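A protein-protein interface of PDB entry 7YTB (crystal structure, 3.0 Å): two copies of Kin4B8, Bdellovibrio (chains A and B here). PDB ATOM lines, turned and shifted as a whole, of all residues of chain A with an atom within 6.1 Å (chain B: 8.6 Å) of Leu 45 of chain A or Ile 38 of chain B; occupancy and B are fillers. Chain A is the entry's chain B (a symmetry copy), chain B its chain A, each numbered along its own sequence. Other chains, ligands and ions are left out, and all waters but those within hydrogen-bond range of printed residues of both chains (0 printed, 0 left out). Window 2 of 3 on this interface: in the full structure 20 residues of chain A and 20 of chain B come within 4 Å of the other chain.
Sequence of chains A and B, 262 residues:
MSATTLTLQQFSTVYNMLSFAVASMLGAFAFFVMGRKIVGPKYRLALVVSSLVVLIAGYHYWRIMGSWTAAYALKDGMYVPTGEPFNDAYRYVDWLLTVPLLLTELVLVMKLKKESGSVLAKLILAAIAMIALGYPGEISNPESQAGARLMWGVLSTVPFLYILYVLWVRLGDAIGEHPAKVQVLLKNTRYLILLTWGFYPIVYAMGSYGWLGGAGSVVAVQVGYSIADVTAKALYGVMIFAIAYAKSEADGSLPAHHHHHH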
ATOM      1  N   ARG A  36      -0.306  21.918  29.146  1.00  0.00           N
ATOM      2  CA  ARG A  36      -0.401  22.077  27.696  1.00  0.00           C
ATOM      3  C   ARG A  36       0.451  21.053  26.953  1.00  0.00           C
ATOM      4  O   ARG A  36       0.044  20.544  25.902  1.00  0.00           O
ATOM      5  CB  ARG A  36       0.008  23.496  27.297  1.00  0.00           C
ATOM      6  CG  ARG A  36      -0.924  24.596  27.782  1.00  0.00           C
ATOM      7  CD  ARG A  36      -0.437  25.964  27.312  1.00  0.00           C
ATOM      8  NE  ARG A  36       0.898  26.269  27.815  1.00  0.00           N
ATOM      9  CZ  ARG A  36       1.692  27.209  27.316  1.00  0.00           C
ATOM     10  NH1 ARG A  36       1.328  27.943  26.276  1.00  0.00           N
ATOM     11  NH2 ARG A  36       2.884  27.411  27.871  1.00  0.00           N
ATOM     12  N   PRO A  41      -2.218  18.891  20.110  1.00  0.00           N
ATOM     13  CA  PRO A  41      -2.053  20.315  19.776  1.00  0.00           C
ATOM     14  C   PRO A  41      -3.352  21.029  19.442  1.00  0.00           C
ATOM     15  O   PRO A  41      -3.405  22.260  19.555  1.00  0.00           O
ATOM     16  CB  PRO A  41      -1.103  20.284  18.569  1.00  0.00           C
ATOM     17  CG  PRO A  41      -0.408  18.953  18.677  1.00  0.00           C
ATOM     18  CD  PRO A  41      -1.459  18.024  19.199  1.00  0.00           C
ATOM     19  N   LYS A  42      -4.397  20.312  19.046  1.00  0.00           N
ATOM     20  CA  LYS A  42      -5.645  20.953  18.658  1.00  0.00           C
ATOM     21  C   LYS A  42      -6.533  21.255  19.857  1.00  0.00           C
ATOM     22  O   LYS A  42      -7.585  21.879  19.689  1.00  0.00           O
ATOM     23  CB  LYS A  42      -6.395  20.051  17.681  1.00  0.00           C
ATOM     24  CG  LYS A  42      -5.505  19.432  16.629  1.00  0.00           C
ATOM     25  CD  LYS A  42      -5.927  18.002  16.368  1.00  0.00           C
ATOM     26  CE  LYS A  42      -5.832  17.205  17.663  1.00  0.00           C
ATOM     27  NZ  LYS A  42      -4.503  17.367  18.314  1.00  0.00           N
ATOM     28  N   TYR A  43      -6.137  20.822  21.055  1.00  0.00           N
ATOM     29  CA  TYR A  43      -6.874  21.077  22.284  1.00  0.00           C
ATOM     30  C   TYR A  43      -6.127  21.998  23.238  1.00  0.00           C
ATOM     31  O   TYR A  43      -6.597  22.222  24.358  1.00  0.00           O
ATOM     32  CB  TYR A  43      -7.197  19.754  22.988  1.00  0.00           C
ATOM     33  CG  TYR A  43      -7.893  18.741  22.105  1.00  0.00           C
ATOM     34  CD1 TYR A  43      -9.246  18.861  21.814  1.00  0.00           C
ATOM     35  CD2 TYR A  43      -7.197  17.674  21.555  1.00  0.00           C
ATOM     36  CE1 TYR A  43      -9.887  17.938  21.008  1.00  0.00           C
ATOM     37  CE2 TYR A  43      -7.829  16.745  20.750  1.00  0.00           C
ATOM     38  CZ  TYR A  43      -9.174  16.883  20.478  1.00  0.00           C
ATOM     39  OH  TYR A  43      -9.807  15.964  19.676  1.00  0.00           O
ATOM     40  N   ARG A  44      -4.979  22.540  22.827  1.00  0.00           N
ATOM     41  CA  ARG A  44      -4.168  23.335  23.741  1.00  0.00           C
ATOM     42  C   ARG A  44      -4.714  24.746  23.916  1.00  0.00           C
ATOM     43  O   ARG A  44      -4.507  25.360  24.968  1.00  0.00           O
ATOM     44  CB  ARG A  44      -2.717  23.375  23.256  1.00  0.00           C
ATOM     45  CG  ARG A  44      -1.999  22.041  23.378  1.00  0.00           C
ATOM     46  CD  ARG A  44      -0.604  22.077  22.771  1.00  0.00           C
ATOM     47  NE  ARG A  44       0.009  20.752  22.741  1.00  0.00           N
ATOM     48  CZ  ARG A  44       1.173  20.472  22.168  1.00  0.00           C
ATOM     49  NH1 ARG A  44       1.902  21.409  21.585  1.00  0.00           N
ATOM     50  NH2 ARG A  44       1.620  19.219  22.190  1.00  0.00           N
ATOM     51  N   LEU A  45      -5.404  25.274  22.901  1.00  0.00           N
ATOM     52  CA  LEU A  45      -6.022  26.590  23.025  1.00  0.00           C
ATOM     53  C   LEU A  45      -7.109  26.600  24.087  1.00  0.00           C
ATOM     54  O   LEU A  45      -7.305  27.612  24.766  1.00  0.00           O
ATOM     55  CB  LEU A  45      -6.600  27.027  21.679  1.00  0.00           C
ATOM     56  CG  LEU A  45      -7.048  28.484  21.561  1.00  0.00           C
ATOM     57  CD1 LEU A  45      -5.883  29.426  21.820  1.00  0.00           C
ATOM     58  CD2 LEU A  45      -7.668  28.743  20.192  1.00  0.00           C
ATOM     59  N   ALA A  46      -7.824  25.485  24.241  1.00  0.00           N
ATOM     60  CA  ALA A  46      -8.842  25.395  25.281  1.00  0.00           C
ATOM     61  C   ALA A  46      -8.224  25.454  26.673  1.00  0.00           C
ATOM     62  O   ALA A  46      -8.813  26.025  27.597  1.00  0.00           O
ATOM     63  CB  ALA A  46      -9.656  24.116  25.103  1.00  0.00           C
ATOM     64  N   LEU A  47      -7.041  24.856  26.847  1.00  0.00           N
ATOM     65  CA  LEU A  47      -6.371  24.911  28.143  1.00  0.00           C
ATOM     66  C   LEU A  47      -5.835  26.305  28.447  1.00  0.00           C
ATOM     67  O   LEU A  47      -5.752  26.691  29.620  1.00  0.00           O
ATOM     68  CB  LEU A  47      -5.229  23.894  28.187  1.00  0.00           C
ATOM     69  CG  LEU A  47      -5.543  22.403  28.069  1.00  0.00           C
ATOM     70  CD1 LEU A  47      -4.339  21.583  28.518  1.00  0.00           C
ATOM     71  CD2 LEU A  47      -6.780  22.040  28.870  1.00  0.00           C
ATOM     72  N   VAL A  48      -5.445  27.058  27.416  1.00  0.00           N
ATOM     73  CA  VAL A  48      -5.018  28.439  27.620  1.00  0.00           C
ATOM     74  C   VAL A  48      -6.164  29.265  28.184  1.00  0.00           C
ATOM     75  O   VAL A  48      -5.987  30.053  29.122  1.00  0.00           O
ATOM     76  CB  VAL A  48      -4.482  29.035  26.306  1.00  0.00           C
ATOM     77  CG1 VAL A  48      -4.393  30.547  26.412  1.00  0.00           C
ATOM     78  CG2 VAL A  48      -3.127  28.449  25.979  1.00  0.00           C
ATOM     79  N   VAL A  49      -7.362  29.096  27.615  1.00  0.00           N
ATOM     80  CA  VAL A  49      -8.535  29.800  28.124  1.00  0.00           C
ATOM     81  C   VAL A  49      -8.856  29.339  29.539  1.00  0.00           C
ATOM     82  O   VAL A  49      -9.298  30.135  30.377  1.00  0.00           O
ATOM     83  CB  VAL A  49      -9.730  29.598  27.170  1.00  0.00           C
ATOM     84  CG1 VAL A  49     -10.980  30.258  27.723  1.00  0.00           C
ATOM     85  CG2 VAL A  49      -9.409  30.149  25.791  1.00  0.00           C
ATOM     86  N   SER A  50      -8.643  28.053  29.829  1.00  0.00           N
ATOM     87  CA  SER A  50      -8.811  27.554  31.191  1.00  0.00           C
ATOM     88  C   SER A  50      -7.882  28.280  32.155  1.00  0.00           C
ATOM     89  O   SER A  50      -8.294  28.695  33.244  1.00  0.00           O
ATOM     90  CB  SER A  50      -8.556  26.047  31.232  1.00  0.00           C
ATOM     91  OG  SER A  50      -9.505  25.344  30.450  1.00  0.00           O
ATOM     92  N   LEU A 108     -14.222  25.018  22.728  1.00  0.00           N
ATOM     93  CA  LEU A 108     -12.941  24.767  22.077  1.00  0.00           C
ATOM     94  C   LEU A 108     -12.458  23.341  22.299  1.00  0.00           C
ATOM     95  O   LEU A 108     -11.813  22.769  21.413  1.00  0.00           O
ATOM     96  CB  LEU A 108     -11.889  25.758  22.571  1.00  0.00           C
ATOM     97  CG  LEU A 108     -12.085  27.222  22.176  1.00  0.00           C
ATOM     98  CD1 LEU A 108     -10.869  28.038  22.583  1.00  0.00           C
ATOM     99  CD2 LEU A 108     -12.351  27.341  20.683  1.00  0.00           C
ATOM    100  N   PHE B  31      -2.626  35.426  27.518  1.00  0.00           N
ATOM    101  CA  PHE B  31      -3.065  34.849  26.249  1.00  0.00           C
ATOM    102  C   PHE B  31      -2.040  35.079  25.144  1.00  0.00           C
ATOM    103  O   PHE B  31      -1.670  34.147  24.424  1.00  0.00           O
ATOM    104  CB  PHE B  31      -4.423  35.436  25.860  1.00  0.00           C
ATOM    105  CG  PHE B  31      -4.986  34.881  24.581  1.00  0.00           C
ATOM    106  CD1 PHE B  31      -5.478  33.587  24.523  1.00  0.00           C
ATOM    107  CD2 PHE B  31      -5.039  35.665  23.438  1.00  0.00           C
ATOM    108  CE1 PHE B  31      -5.995  33.080  23.342  1.00  0.00           C
ATOM    109  CE2 PHE B  31      -5.556  35.166  22.259  1.00  0.00           C
ATOM    110  CZ  PHE B  31      -6.036  33.873  22.211  1.00  0.00           C
ATOM    111  N   PHE B  32      -1.579  36.320  24.986  1.00  0.00           N
ATOM    112  CA  PHE B  32      -0.650  36.631  23.903  1.00  0.00           C
ATOM    113  C   PHE B  32       0.704  35.969  24.119  1.00  0.00           C
ATOM    114  O   PHE B  32       1.346  35.530  23.158  1.00  0.00           O
ATOM    115  CB  PHE B  32      -0.496  38.146  23.763  1.00  0.00           C
ATOM    116  CG  PHE B  32      -1.793  38.863  23.518  1.00  0.00           C
ATOM    117  CD1 PHE B  32      -2.798  38.265  22.771  1.00  0.00           C
ATOM    118  CD2 PHE B  32      -2.017  40.122  24.044  1.00  0.00           C
ATOM    119  CE1 PHE B  32      -3.994  38.920  22.547  1.00  0.00           C
ATOM    120  CE2 PHE B  32      -3.211  40.779  23.826  1.00  0.00           C
ATOM    121  CZ  PHE B  32      -4.201  40.176  23.077  1.00  0.00           C
ATOM    122  N   VAL B  33       1.159  35.896  25.372  1.00  0.00           N
ATOM    123  CA  VAL B  33       2.411  35.205  25.672  1.00  0.00           C
ATOM    124  C   VAL B  33       2.298  33.723  25.328  1.00  0.00           C
ATOM    125  O   VAL B  33       3.171  33.152  24.662  1.00  0.00           O
ATOM    126  CB  VAL B  33       2.800  35.416  27.147  1.00  0.00           C
ATOM    127  CG1 VAL B  33       3.997  34.558  27.510  1.00  0.00           C
ATOM    128  CG2 VAL B  33       3.105  36.878  27.411  1.00  0.00           C
ATOM    129  N   MET B  34       1.214  33.079  25.770  1.00  0.00           N
ATOM    130  CA  MET B  34       1.020  31.661  25.486  1.00  0.00           C
ATOM    131  C   MET B  34       0.593  31.414  24.044  1.00  0.00           C
ATOM    132  O   MET B  34       0.960  30.386  23.462  1.00  0.00           O
ATOM    133  CB  MET B  34       0.008  31.063  26.463  1.00  0.00           C
ATOM    134  CG  MET B  34       0.552  30.906  27.877  1.00  0.00           C
ATOM    135  SD  MET B  34      -0.596  30.141  29.043  1.00  0.00           S
ATOM    136  CE  MET B  34      -1.586  31.554  29.525  1.00  0.00           C
ATOM    137  N   GLY B  35      -0.183  32.326  23.453  1.00  0.00           N
ATOM    138  CA  GLY B  35      -0.602  32.138  22.075  1.00  0.00           C
ATOM    139  C   GLY B  35       0.516  32.300  21.070  1.00  0.00           C
ATOM    140  O   GLY B  35       0.345  31.923  19.905  1.00  0.00           O
ATOM    141  N   ARG B  36       1.648  32.861  21.501  1.00  0.00           N
ATOM    142  CA  ARG B  36       2.812  32.987  20.633  1.00  0.00           C
ATOM    143  C   ARG B  36       3.268  31.618  20.142  1.00  0.00           C
ATOM    144  O   ARG B  36       3.655  31.458  18.980  1.00  0.00           O
ATOM    145  CB  ARG B  36       3.923  33.691  21.410  1.00  0.00           C
ATOM    146  CG  ARG B  36       5.043  34.259  20.584  1.00  0.00           C
ATOM    147  CD  ARG B  36       5.992  35.067  21.462  1.00  0.00           C
ATOM    148  NE  ARG B  36       6.766  34.229  22.370  1.00  0.00           N
ATOM    149  CZ  ARG B  36       6.572  34.153  23.680  1.00  0.00           C
ATOM    150  NH1 ARG B  36       5.642  34.875  24.285  1.00  0.00           N
ATOM    151  NH2 ARG B  36       7.334  33.337  24.403  1.00  0.00           N
ATOM    152  N   LYS B  37       3.234  30.623  21.028  1.00  0.00           N
ATOM    153  CA  LYS B  37       3.655  29.266  20.707  1.00  0.00           C
ATOM    154  C   LYS B  37       2.692  28.555  19.762  1.00  0.00           C
ATOM    155  O   LYS B  37       3.077  27.558  19.142  1.00  0.00           O
ATOM    156  CB  LYS B  37       3.838  28.499  22.015  1.00  0.00           C
ATOM    157  CG  LYS B  37       4.813  29.229  22.926  1.00  0.00           C
ATOM    158  CD  LYS B  37       4.651  28.880  24.386  1.00  0.00           C
ATOM    159  CE  LYS B  37       4.805  30.137  25.236  1.00  0.00           C
ATOM    160  NZ  LYS B  37       4.689  29.858  26.689  1.00  0.00           N
ATOM    161  N   ILE B  38       1.456  29.041  19.634  1.00  0.00           N
ATOM    162  CA  ILE B  38       0.425  28.322  18.891  1.00  0.00           C
ATOM    163  C   ILE B  38       0.351  28.726  17.418  1.00  0.00           C
ATOM    164  O   ILE B  38      -0.126  27.936  16.590  1.00  0.00           O
ATOM    165  CB  ILE B  38      -0.942  28.516  19.580  1.00  0.00           C
ATOM    166  CG1 ILE B  38      -0.914  27.921  20.990  1.00  0.00           C
ATOM    167  CG2 ILE B  38      -2.080  27.880  18.789  1.00  0.00           C
ATOM    168  CD1 ILE B  38      -2.258  27.954  21.686  1.00  0.00           C
ATOM    169  N   VAL B  39       0.811  29.918  17.062  1.00  0.00           N
ATOM    170  CA  VAL B  39       0.734  30.397  15.695  1.00  0.00           C
ATOM    171  C   VAL B  39       2.077  30.171  14.996  1.00  0.00           C
ATOM    172  O   VAL B  39       3.051  29.737  15.603  1.00  0.00           O
ATOM    173  CB  VAL B  39       0.308  31.882  15.629  1.00  0.00           C
ATOM    174  CG1 VAL B  39      -1.117  32.040  16.137  1.00  0.00           C
ATOM    175  CG2 VAL B  39       1.270  32.744  16.432  1.00  0.00           C
ATOM    176  N   GLY B  40       2.118  30.471  13.700  1.00  0.00           N
ATOM    177  CA  GLY B  40       3.307  30.292  12.896  1.00  0.00           C
ATOM    178  C   GLY B  40       4.461  31.166  13.341  1.00  0.00           C
ATOM    179  O   GLY B  40       4.279  32.179  14.021  1.00  0.00           O
ATOM    180  N   PRO B  41       5.684  30.777  12.969  1.00  0.00           N
ATOM    181  CA  PRO B  41       6.866  31.483  13.491  1.00  0.00           C
ATOM    182  C   PRO B  41       7.001  32.919  13.012  1.00  0.00           C
ATOM    183  O   PRO B  41       7.632  33.723  13.710  1.00  0.00           O
ATOM    184  CB  PRO B  41       8.039  30.626  12.983  1.00  0.00           C
ATOM    185  CG  PRO B  41       7.426  29.288  12.669  1.00  0.00           C
ATOM    186  CD  PRO B  41       6.063  29.624  12.141  1.00  0.00           C
ATOM    187  N   TYR B  43       4.605  35.160  12.654  1.00  0.00           N
ATOM    188  CA  TYR B  43       3.595  36.045  13.218  1.00  0.00           C
ATOM    189  C   TYR B  43       3.783  36.245  14.716  1.00  0.00           C
ATOM    190  O   TYR B  43       2.941  36.878  15.361  1.00  0.00           O
ATOM    191  CB  TYR B  43       2.193  35.497  12.943  1.00  0.00           C
ATOM    192  CG  TYR B  43       1.936  35.149  11.494  1.00  0.00           C
ATOM    193  CD1 TYR B  43       1.695  36.139  10.551  1.00  0.00           C
ATOM    194  CD2 TYR B  43       1.914  33.826  11.074  1.00  0.00           C
ATOM    195  CE1 TYR B  43       1.450  35.820   9.224  1.00  0.00           C
ATOM    196  CE2 TYR B  43       1.669  33.499   9.751  1.00  0.00           C
ATOM    197  CZ  TYR B  43       1.439  34.498   8.830  1.00  0.00           C
ATOM    198  OH  TYR B  43       1.198  34.160   7.517  1.00  0.00           O
ATOM    199  N   ARG B  44       4.866  35.712  15.282  1.00  0.00           N
ATOM    200  CA  ARG B  44       5.053  35.742  16.727  1.00  0.00           C
ATOM    201  C   ARG B  44       5.560  37.086  17.229  1.00  0.00           C
ATOM    202  O   ARG B  44       5.295  37.449  18.381  1.00  0.00           O
ATOM    203  CB  ARG B  44       6.004  34.624  17.149  1.00  0.00           C
ATOM    204  CG  ARG B  44       5.395  33.245  16.996  1.00  0.00           C
ATOM    205  CD  ARG B  44       6.389  32.134  17.285  1.00  0.00           C
ATOM    206  NE  ARG B  44       5.824  30.825  16.974  1.00  0.00           N
ATOM    207  CZ  ARG B  44       6.496  29.682  17.018  1.00  0.00           C
ATOM    208  NH1 ARG B  44       7.769  29.641  17.377  1.00  0.00           N
ATOM    209  NH2 ARG B  44       5.871  28.551  16.707  1.00  0.00           N
ATOM    210  N   LEU B  47       2.618  39.096  18.080  1.00  0.00           N
ATOM    211  CA  LEU B  47       2.079  38.745  19.389  1.00  0.00           C
ATOM    212  C   LEU B  47       2.975  39.253  20.512  1.00  0.00           C
ATOM    213  O   LEU B  47       2.483  39.548  21.607  1.00  0.00           O
ATOM    214  CB  LEU B  47       1.876  37.232  19.498  1.00  0.00           C
ATOM    215  CG  LEU B  47       0.843  36.619  18.549  1.00  0.00           C
ATOM    216  CD1 LEU B  47       0.431  35.231  19.010  1.00  0.00           C
ATOM    217  CD2 LEU B  47      -0.371  37.523  18.444  1.00  0.00           C
ATOM    218  N   PHE B 241      -4.306  38.045  17.042  1.00  0.00           N
ATOM    219  CA  PHE B 241      -4.045  36.620  17.202  1.00  0.00           C
ATOM    220  C   PHE B 241      -4.875  35.790  16.230  1.00  0.00           C
ATOM    221  O   PHE B 241      -4.373  34.826  15.639  1.00  0.00           O
ATOM    222  CB  PHE B 241      -4.331  36.187  18.638  1.00  0.00           C
ATOM    223  CG  PHE B 241      -4.221  34.707  18.854  1.00  0.00           C
ATOM    224  CD1 PHE B 241      -2.994  34.118  19.093  1.00  0.00           C
ATOM    225  CD2 PHE B 241      -5.350  33.904  18.813  1.00  0.00           C
ATOM    226  CE1 PHE B 241      -2.896  32.755  19.291  1.00  0.00           C
ATOM    227  CE2 PHE B 241      -5.258  32.543  19.010  1.00  0.00           C
ATOM    228  CZ  PHE B 241      -4.031  31.968  19.250  1.00  0.00           C
ATOM    229  N   ALA B 242      -6.152  36.142  16.064  1.00  0.00           N
ATOM    230  CA  ALA B 242      -7.016  35.380  15.168  1.00  0.00           C
ATOM    231  C   ALA B 242      -6.544  35.490  13.725  1.00  0.00           C
ATOM    232  O   ALA B 242      -6.618  34.518  12.964  1.00  0.00           O
ATOM    233  CB  ALA B 242      -8.460  35.857  15.304  1.00  0.00           C
ATOM    234  N   ALA B 244      -3.394  35.976  12.949  1.00  0.00           N
ATOM    235  CA  ALA B 244      -2.180  35.169  12.945  1.00  0.00           C
ATOM    236  C   ALA B 244      -2.504  33.684  12.838  1.00  0.00           C
ATOM    237  O   ALA B 244      -1.849  32.952  12.090  1.00  0.00           O
ATOM    238  CB  ALA B 244      -1.359  35.452  14.201  1.00  0.00           C
ATOM    239  N   TYR B 245      -3.515  33.223  13.580  1.00  0.00           N
ATOM    240  CA  TYR B 245      -3.887  31.812  13.543  1.00  0.00           C
ATOM    241  C   TYR B 245      -4.432  31.413  12.178  1.00  0.00           C
ATOM    242  O   TYR B 245      -4.141  30.316  11.685  1.00  0.00           O
ATOM    243  CB  TYR B 245      -4.919  31.518  14.635  1.00  0.00           C
ATOM    244  CG  TYR B 245      -5.309  30.061  14.763  1.00  0.00           C
ATOM    245  CD1 TYR B 245      -6.316  29.514  13.976  1.00  0.00           C
ATOM    246  CD2 TYR B 245      -4.676  29.232  15.678  1.00  0.00           C
ATOM    247  CE1 TYR B 245      -6.674  28.183  14.095  1.00  0.00           C
ATOM    248  CE2 TYR B 245      -5.030  27.898  15.804  1.00  0.00           C
ATOM    249  CZ  TYR B 245      -6.029  27.380  15.010  1.00  0.00           C
ATOM    250  OH  TYR B 245      -6.381  26.055  15.136  1.00  0.00           O
ATOM    251  N   ALA B 246      -5.229  32.284  11.558  1.00  0.00           N
ATOM    252  CA  ALA B 246      -5.788  31.968  10.248  1.00  0.00           C
ATOM    253  C   ALA B 246      -4.702  31.907   9.183  1.00  0.00           C
ATOM    254  O   ALA B 246      -4.686  30.988   8.355  1.00  0.00           O
ATOM    255  CB  ALA B 246      -6.855  32.994   9.872  1.00  0.00           C
ATOM    256  N   SER B 248      -1.569  31.294   9.706  1.00  0.00           N
ATOM    257  CA  SER B 248      -0.735  30.130   9.991  1.00  0.00           C
ATOM    258  C   SER B 248      -1.377  28.841   9.486  1.00  0.00           C
ATOM    259  O   SER B 248      -0.677  27.938   9.013  1.00  0.00           O
ATOM    260  CB  SER B 248      -0.459  30.036  11.492  1.00  0.00           C
ATOM    261  OG  SER B 248       0.332  31.124  11.937  1.00  0.00           O
ATOM    262  N   GLU B 249      -2.705  28.734   9.579  1.00  0.00           N
ATOM    263  CA  GLU B 249      -3.383  27.562   9.040  1.00  0.00           C
ATOM    264  C   GLU B 249      -3.394  27.578   7.519  1.00  0.00           C
ATOM    265  O   GLU B 249      -3.538  26.521   6.895  1.00  0.00           O
ATOM    266  CB  GLU B 249      -4.815  27.476   9.577  1.00  0.00           C
ATOM    267  CG  GLU B 249      -5.521  26.156   9.276  1.00  0.00           C
ATOM    268  CD  GLU B 249      -6.902  26.062   9.900  1.00  0.00           C
ATOM    269  OE1 GLU B 249      -7.357  27.051  10.512  1.00  0.00           O
ATOM    270  OE2 GLU B 249      -7.534  24.989   9.785  1.00  0.00           O
ATOM    271  N   SER B 253       2.043  26.703   8.370  1.00  0.00           N
ATOM    272  CA  SER B 253       3.038  26.913   9.412  1.00  0.00           C
ATOM    273  C   SER B 253       2.463  26.746  10.808  1.00  0.00           C
ATOM    274  O   SER B 253       3.182  26.975  11.787  1.00  0.00           O
ATOM    275  CB  SER B 253       3.666  28.303   9.278  1.00  0.00           C
ATOM    276  OG  SER B 253       2.673  29.311   9.290  1.00  0.00           O
ATOM    277  N   LEU B 254       1.189  26.384  10.921  1.00  0.00           N
ATOM    278  CA  LEU B 254       0.579  26.117  12.211  1.00  0.00           C
ATOM    279  C   LEU B 254       1.400  25.052  12.939  1.00  0.00           C
ATOM    280  O   LEU B 254       1.572  23.945  12.409  1.00  0.00           O
ATOM    281  CB  LEU B 254      -0.867  25.658  12.032  1.00  0.00           C
ATOM    282  CG  LEU B 254      -1.818  25.822  13.222  1.00  0.00           C
ATOM    283  CD1 LEU B 254      -1.779  27.243  13.767  1.00  0.00           C
ATOM    284  CD2 LEU B 254      -3.239  25.452  12.823  1.00  0.00           C
ATOM    285  N   PRO B 255       1.941  25.359  14.123  1.00  0.00           N
ATOM    286  CA  PRO B 255       2.789  24.392  14.845  1.00  0.00           C
ATOM    287  C   PRO B 255       2.216  22.994  14.982  1.00  0.00           C
ATOM    288  O   PRO B 255       2.985  22.048  15.191  1.00  0.00           O
ATOM    289  CB  PRO B 255       2.955  25.058  16.216  1.00  0.00           C
ATOM    290  CG  PRO B 255       2.899  26.507  15.919  1.00  0.00           C
ATOM    291  CD  PRO B 255       1.924  26.676  14.778  1.00  0.00           C
ATOM    292  N   ALA B 256       0.903  22.827  14.860  1.00  0.00           N
ATOM    293  CA  ALA B 256       0.287  21.514  15.000  1.00  0.00           C
ATOM    294  C   ALA B 256       0.750  20.577  13.888  1.00  0.00           C
ATOM    295  O   ALA B 256       0.191  20.570  12.792  1.00  0.00           O
ATOM    296  CB  ALA B 256      -1.229  21.640  14.993  1.00  0.00           C
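Among the printed residues, pairs that only touch across the chains: Arg 36 of chain A with Met 34 of chain B, Pro 41 of chain A with Ala 256 of chain B, Leu 45 of chain A with Phe 31 of chain B, Leu 45 of chain A with Ile 38 of chain B and Val 48 of chain A with Phe 31 of chain B.
Positions printed for both chains: 36, 41, 43, 44 and 47.
NZ of Lys 37 of chain B lies close to NH2 of Arg 36 of chain A (3.3 Å).
Of the 12 printed residues of chain A, 4 touch a printed residue of chain B. Among the printed residues, no Asp or Glu carboxylate lies within 4 Å of a Lys or Arg side-chain nitrogen of the other chain.
NE of Arg 44 of chain A is in hydrogen-bond range of O of Arg 36 of chain A (3.2 Å).
Printed residues of chain B within 4 Å of Leu 45 of chain A: Phe 31 (3.96 Å) and Ile 38 (3.9 Å). Ile 38 of chain B touches one residue of chain A. No residue of chain B comes within 4 Å of Ala 46 of chain A. Printed residues of chain B within 4 Å of Val 48 of chain A: Phe 31 (3.7 Å). Of the printed residues of chain A, Met 34 of chain B touches Arg 36 (3.4 Å). Of the printed residues of chain B, Arg 36 of chain A touches Met 34 (3.4 Å) and Lys 37 (3.3 Å). Of the printed residues of chain A, Phe 31 of chain B touches Leu 45 (3.96 Å) and Val 48 (3.7 Å). Of the printed residues of chain B, Pro 41 of chain A touches Ala 256 (3.8 Å). The nearest printed residue of chain B that does not touch Val 48 of chain A is Met 34 of chain B (4.1 Å).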
